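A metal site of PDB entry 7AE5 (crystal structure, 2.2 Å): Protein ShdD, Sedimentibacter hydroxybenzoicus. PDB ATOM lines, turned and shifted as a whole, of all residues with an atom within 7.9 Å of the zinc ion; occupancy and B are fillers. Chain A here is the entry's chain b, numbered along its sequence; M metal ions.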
ATOM      1  N   LYS A   2      30.286 -10.626 -21.907  1.00  0.00           N
ATOM      2  CA  LYS A   2      29.263 -11.148 -21.017  1.00  0.00           C
ATOM      3  C   LYS A   2      29.725 -11.037 -19.572  1.00  0.00           C
ATOM      4  O   LYS A   2      30.920 -11.009 -19.279  1.00  0.00           O
ATOM      5  CB  LYS A   2      28.938 -12.602 -21.359  1.00  0.00           C
ATOM      6  N   CYS A   3      28.750 -10.970 -18.664  1.00  0.00           N
ATOM      7  CA  CYS A   3      29.057 -10.933 -17.233  1.00  0.00           C
ATOM      8  C   CYS A   3      29.457 -12.322 -16.751  1.00  0.00           C
ATOM      9  O   CYS A   3      28.759 -13.309 -17.026  1.00  0.00           O
ATOM     10  CB  CYS A   3      27.868 -10.422 -16.435  1.00  0.00           C
ATOM     11  SG  CYS A   3      28.109 -10.520 -14.641  1.00  0.00           S
ATOM     12  N   HIS A   4      30.583 -12.395 -16.041  1.00  0.00           N
ATOM     13  CA  HIS A   4      31.084 -13.681 -15.585  1.00  0.00           C
ATOM     14  C   HIS A   4      30.205 -14.309 -14.506  1.00  0.00           C
ATOM     15  O   HIS A   4      30.263 -15.523 -14.302  1.00  0.00           O
ATOM     16  CB  HIS A   4      32.519 -13.534 -15.059  1.00  0.00           C
ATOM     17  CG  HIS A   4      33.516 -13.215 -16.124  1.00  0.00           C
ATOM     18  ND1 HIS A   4      33.702 -11.948 -16.623  1.00  0.00           N
ATOM     19  CD2 HIS A   4      34.396 -14.014 -16.781  1.00  0.00           C
ATOM     20  CE1 HIS A   4      34.641 -11.975 -17.553  1.00  0.00           C
ATOM     21  NE2 HIS A   4      35.084 -13.222 -17.663  1.00  0.00           N
ATOM     22  N   ARG A   5      29.387 -13.513 -13.823  1.00  0.00           N
ATOM     23  CA  ARG A   5      28.540 -14.014 -12.746  1.00  0.00           C
ATOM     24  C   ARG A   5      27.122 -14.323 -13.186  1.00  0.00           C
ATOM     25  O   ARG A   5      26.581 -15.366 -12.796  1.00  0.00           O
ATOM     26  CB  ARG A   5      28.498 -12.994 -11.591  1.00  0.00           C
ATOM     27  CG  ARG A   5      27.723 -13.502 -10.383  1.00  0.00           C
ATOM     28  CD  ARG A   5      28.162 -12.804  -9.107  1.00  0.00           C
ATOM     29  NE  ARG A   5      27.823 -11.387  -9.090  1.00  0.00           N
ATOM     30  CZ  ARG A   5      27.908 -10.603  -8.019  1.00  0.00           C
ATOM     31  NH1 ARG A   5      28.309 -11.078  -6.857  1.00  0.00           N
ATOM     32  NH2 ARG A   5      27.579  -9.322  -8.122  1.00  0.00           N
ATOM     33  N   CYS A   6      26.495 -13.454 -13.974  1.00  0.00           N
ATOM     34  CA  CYS A   6      25.092 -13.612 -14.329  1.00  0.00           C
ATOM     35  C   CYS A   6      24.841 -13.759 -15.828  1.00  0.00           C
ATOM     36  O   CYS A   6      23.697 -13.954 -16.229  1.00  0.00           O
ATOM     37  CB  CYS A   6      24.277 -12.436 -13.788  1.00  0.00           C
ATOM     38  SG  CYS A   6      24.434 -10.923 -14.764  1.00  0.00           S
ATOM     39  N   GLY A   7      25.888 -13.677 -16.656  1.00  0.00           N
ATOM     40  CA  GLY A   7      25.724 -13.884 -18.078  1.00  0.00           C
ATOM     41  C   GLY A   7      25.074 -12.746 -18.843  1.00  0.00           C
ATOM     42  O   GLY A   7      24.838 -12.895 -20.045  1.00  0.00           O
ATOM     43  N   SER A   8      24.772 -11.627 -18.194  1.00  0.00           N
ATOM     44  CA  SER A   8      24.200 -10.495 -18.905  1.00  0.00           C
ATOM     45  C   SER A   8      25.250  -9.838 -19.793  1.00  0.00           C
ATOM     46  O   SER A   8      26.455  -9.891 -19.527  1.00  0.00           O
ATOM     47  CB  SER A   8      23.644  -9.466 -17.916  1.00  0.00           C
ATOM     48  OG  SER A   8      23.561  -8.187 -18.514  1.00  0.00           O
ATOM     49  N   ASP A   9      24.776  -9.221 -20.870  1.00  0.00           N
ATOM     50  CA  ASP A   9      25.627  -8.456 -21.771  1.00  0.00           C
ATOM     51  C   ASP A   9      25.604  -6.964 -21.467  1.00  0.00           C
ATOM     52  O   ASP A   9      26.300  -6.198 -22.144  1.00  0.00           O
ATOM     53  CB  ASP A   9      25.214  -8.697 -23.226  1.00  0.00           C
ATOM     54  N   ASN A  10      24.836  -6.537 -20.469  1.00  0.00           N
ATOM     55  CA  ASN A  10      24.740  -5.129 -20.087  1.00  0.00           C
ATOM     56  C   ASN A  10      25.897  -4.753 -19.149  1.00  0.00           C
ATOM     57  O   ASN A  10      25.697  -4.273 -18.033  1.00  0.00           O
ATOM     58  CB  ASN A  10      23.385  -4.838 -19.453  1.00  0.00           C
ATOM     59  CG  ASN A  10      22.253  -5.511 -20.187  1.00  0.00           C
ATOM     60  OD1 ASN A  10      21.854  -5.090 -21.280  1.00  0.00           O
ATOM     61  ND2 ASN A  10      21.705  -6.573 -19.596  1.00  0.00           N
ATOM     62  N   VAL A  11      27.111  -4.995 -19.623  1.00  0.00           N
ATOM     63  CA  VAL A  11      28.328  -4.636 -18.901  1.00  0.00           C
ATOM     64  C   VAL A  11      28.928  -3.414 -19.574  1.00  0.00           C
ATOM     65  O   VAL A  11      28.963  -3.312 -20.801  1.00  0.00           O
ATOM     66  CB  VAL A  11      29.328  -5.810 -18.873  1.00  0.00           C
ATOM     67  CG1 VAL A  11      29.458  -6.429 -20.251  1.00  0.00           C
ATOM     68  CG2 VAL A  11      30.684  -5.342 -18.369  1.00  0.00           C
ATOM     69  N   VAL A  27      32.019  -3.402 -15.217  1.00  0.00           N
ATOM     70  CA  VAL A  27      30.987  -3.585 -14.198  1.00  0.00           C
ATOM     71  C   VAL A  27      29.685  -3.992 -14.882  1.00  0.00           C
ATOM     72  O   VAL A  27      29.326  -3.451 -15.927  1.00  0.00           O
ATOM     73  CB  VAL A  27      30.784  -2.305 -13.353  1.00  0.00           C
ATOM     74  CG1 VAL A  27      30.663  -1.084 -14.250  1.00  0.00           C
ATOM     75  CG2 VAL A  27      29.586  -2.434 -12.437  1.00  0.00           C
ATOM     76  N   CYS A  28      28.993  -4.961 -14.290  1.00  0.00           N
ATOM     77  CA  CYS A  28      27.713  -5.422 -14.802  1.00  0.00           C
ATOM     78  C   CYS A  28      26.584  -4.580 -14.208  1.00  0.00           C
ATOM     79  O   CYS A  28      26.489  -4.433 -12.985  1.00  0.00           O
ATOM     80  CB  CYS A  28      27.494  -6.900 -14.467  1.00  0.00           C
ATOM     81  SG  CYS A  28      25.828  -7.487 -14.799  1.00  0.00           S
ATOM     82  N   GLU A  29      25.739  -4.031 -15.081  1.00  0.00           N
ATOM     83  CA  GLU A  29      24.647  -3.174 -14.643  1.00  0.00           C
ATOM     84  C   GLU A  29      23.484  -3.939 -14.029  1.00  0.00           C
ATOM     85  O   GLU A  29      22.573  -3.304 -13.479  1.00  0.00           O
ATOM     86  CB  GLU A  29      24.139  -2.327 -15.814  1.00  0.00           C
ATOM     87  CG  GLU A  29      23.946  -0.855 -15.473  1.00  0.00           C
ATOM     88  CD  GLU A  29      23.336  -0.070 -16.625  1.00  0.00           C
ATOM     89  OE1 GLU A  29      23.942   0.934 -17.044  1.00  0.00           O
ATOM     90  OE2 GLU A  29      22.248  -0.458 -17.100  1.00  0.00           O
ATOM     91  N   LYS A  30      23.492  -5.267 -14.095  1.00  0.00           N
ATOM     92  CA  LYS A  30      22.407  -6.078 -13.557  1.00  0.00           C
ATOM     93  C   LYS A  30      22.702  -6.616 -12.161  1.00  0.00           C
ATOM     94  O   LYS A  30      21.812  -6.626 -11.309  1.00  0.00           O
ATOM     95  CB  LYS A  30      22.085  -7.239 -14.500  1.00  0.00           C
ATOM     96  CG  LYS A  30      20.906  -8.082 -14.056  1.00  0.00           C
ATOM     97  CD  LYS A  30      21.181  -9.573 -14.230  1.00  0.00           C
ATOM     98  CE  LYS A  30      20.588 -10.102 -15.522  1.00  0.00           C
ATOM     99  NZ  LYS A  30      20.363 -11.570 -15.464  1.00  0.00           N
ATOM    100  N   CYS A  31      23.941  -7.059 -11.906  1.00  0.00           N
ATOM    101  CA  CYS A  31      24.282  -7.675 -10.632  1.00  0.00           C
ATOM    102  C   CYS A  31      25.456  -7.018  -9.925  1.00  0.00           C
ATOM    103  O   CYS A  31      25.842  -7.478  -8.840  1.00  0.00           O
ATOM    104  CB  CYS A  31      24.583  -9.175 -10.837  1.00  0.00           C
ATOM    105  SG  CYS A  31      26.209  -9.509 -11.544  1.00  0.00           S
ATOM    106  N   CYS A  32      26.050  -5.974 -10.501  1.00  0.00           N
ATOM    107  CA  CYS A  32      27.124  -5.177  -9.897  1.00  0.00           C
ATOM    108  C   CYS A  32      28.446  -5.929  -9.780  1.00  0.00           C
ATOM    109  O   CYS A  32      29.319  -5.526  -9.020  1.00  0.00           O
ATOM    110  CB  CYS A  32      26.728  -4.638  -8.519  1.00  0.00           C
ATOM    111  SG  CYS A  32      25.280  -3.565  -8.526  1.00  0.00           S
ATOM    112  N   TYR A  33      28.621  -7.022 -10.528  1.00  0.00           N
ATOM    113  CA  TYR A  33      29.907  -7.710 -10.544  1.00  0.00           C
ATOM    114  C   TYR A  33      30.931  -6.862 -11.291  1.00  0.00           C
ATOM    115  O   TYR A  33      30.675  -6.392 -12.406  1.00  0.00           O
ATOM    116  CB  TYR A  33      29.789  -9.086 -11.196  1.00  0.00           C
ATOM    117  CG  TYR A  33      31.014  -9.945 -11.033  1.00  0.00           C
ATOM    118  CD1 TYR A  33      31.760 -10.349 -12.137  1.00  0.00           C
ATOM    119  CD2 TYR A  33      31.438 -10.365  -9.774  1.00  0.00           C
ATOM    120  CE1 TYR A  33      32.881 -11.130 -11.999  1.00  0.00           C
ATOM    121  CE2 TYR A  33      32.562 -11.150  -9.627  1.00  0.00           C
ATOM    122  CZ  TYR A  33      33.286 -11.536 -10.741  1.00  0.00           C
ATOM    123  OH  TYR A  33      34.410 -12.320 -10.594  1.00  0.00           O
ATOM    124  N   SER A  34      32.088  -6.657 -10.676  1.00  0.00           N
ATOM    125  CA  SER A  34      33.151  -5.853 -11.252  1.00  0.00           C
ATOM    126  C   SER A  34      34.426  -6.683 -11.396  1.00  0.00           C
ATOM    127  O   SER A  34      34.707  -7.567 -10.576  1.00  0.00           O
ATOM    128  CB  SER A  34      33.440  -4.607 -10.405  1.00  0.00           C
ATOM    129  OG  SER A  34      33.320  -4.882  -9.025  1.00  0.00           O
ATOM    130  N   TRP A  35      35.188  -6.395 -12.452  1.00  0.00           N
ATOM    131  CA  TRP A  35      36.418  -7.123 -12.714  1.00  0.00           C
ATOM    132  C   TRP A  35      37.315  -6.297 -13.618  1.00  0.00           C
ATOM    133  O   TRP A  35      36.831  -5.526 -14.452  1.00  0.00           O
ATOM    134  CB  TRP A  35      36.133  -8.504 -13.335  1.00  0.00           C
ATOM    135  CG  TRP A  35      35.673  -8.453 -14.763  1.00  0.00           C
ATOM    136  CD1 TRP A  35      36.453  -8.554 -15.879  1.00  0.00           C
ATOM    137  CD2 TRP A  35      34.329  -8.325 -15.227  1.00  0.00           C
ATOM    138  NE1 TRP A  35      35.669  -8.477 -17.011  1.00  0.00           N
ATOM    139  CE2 TRP A  35      34.364  -8.334 -16.641  1.00  0.00           C
ATOM    140  CE3 TRP A  35      33.082  -8.184 -14.593  1.00  0.00           C
ATOM    141  CZ2 TRP A  35      33.215  -8.230 -17.422  1.00  0.00           C
ATOM    142  CZ3 TRP A  35      31.940  -8.075 -15.374  1.00  0.00           C
ATOM    143  CH2 TRP A  35      32.018  -8.094 -16.769  1.00  0.00           C
ATOM    144  N   LEU A  49      24.640 -15.999 -10.560  1.00  0.00           N
ATOM    145  CA  LEU A  49      23.327 -15.405 -10.394  1.00  0.00           C
ATOM    146  C   LEU A  49      22.539 -15.508 -11.698  1.00  0.00           C
ATOM    147  O   LEU A  49      23.108 -15.638 -12.780  1.00  0.00           O
ATOM    148  CB  LEU A  49      23.433 -13.938  -9.959  1.00  0.00           C
ATOM    149  CG  LEU A  49      24.115 -13.679  -8.611  1.00  0.00           C
ATOM    150  CD1 LEU A  49      24.290 -12.183  -8.379  1.00  0.00           C
ATOM    151  CD2 LEU A  49      23.329 -14.320  -7.474  1.00  0.00           C
ATOM    152  N   ILE A  54      18.360 -13.121  -8.364  1.00  0.00           N
ATOM    153  CA  ILE A  54      18.432 -11.708  -8.013  1.00  0.00           C
ATOM    154  C   ILE A  54      17.068 -11.202  -7.547  1.00  0.00           C
ATOM    155  O   ILE A  54      16.963 -10.482  -6.555  1.00  0.00           O
ATOM    156  CB  ILE A  54      18.956 -10.877  -9.207  1.00  0.00           C
ATOM    157  CG1 ILE A  54      20.283 -11.443  -9.692  1.00  0.00           C
ATOM    158  CG2 ILE A  54      19.098  -9.420  -8.817  1.00  0.00           C
ATOM    159  CD1 ILE A  54      20.900 -10.644 -10.812  1.00  0.00           C
HETATM  160 ZN    ZN M   1      26.130  -9.595 -13.878  1.00  0.00          ZN
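Of the 21 residues printed, 4 come within 4 Å of the zinc ion.
The nearest printed residue that does not touch the zinc ion is Tyr 33 (4.6 Å).
SG of Cys 3 binds the zinc ion (2.3 Å).
SG of Cys 28 binds the zinc ion (2.3 Å).
The side-chain sulfur (SG) of Cys 6 is bound to the zinc ion, 2.3 Å away.
The zinc ion is bound by SG of Cys 31, 2.3 Å away.
The zinc ion has four donor atoms within binding distance.
The side-chain sulfur (SG) of Cys 3 sits close to the backbone NH (N) of Arg 5 (3.4 Å).
The backbone NH (N) of Cys 3 sits at hydrogen-bond distance from the backbone carbonyl oxygen (O) of Ser 8, 2.7 Å away.
The backbone NH (N) of Cys 28 is in hydrogen-bond range of the backbone carbonyl oxygen (O) of Tyr 33 (2.9 Å).
SG of Cys 28 sits close to N of Lys 30 (3.3 Å).
The side-chain sulfur (SG) of Cys 6 lies close to the backbone NH (N) of Ser 8 (3.5 Å).
SG of Cys 31 lies close to N of Tyr 33 (3.6 Å).
The guanidinium group of Arg 5 lies within hydrogen-bond range of the backbone carbonyl oxygen of Cys 31, 2.6 Å away.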
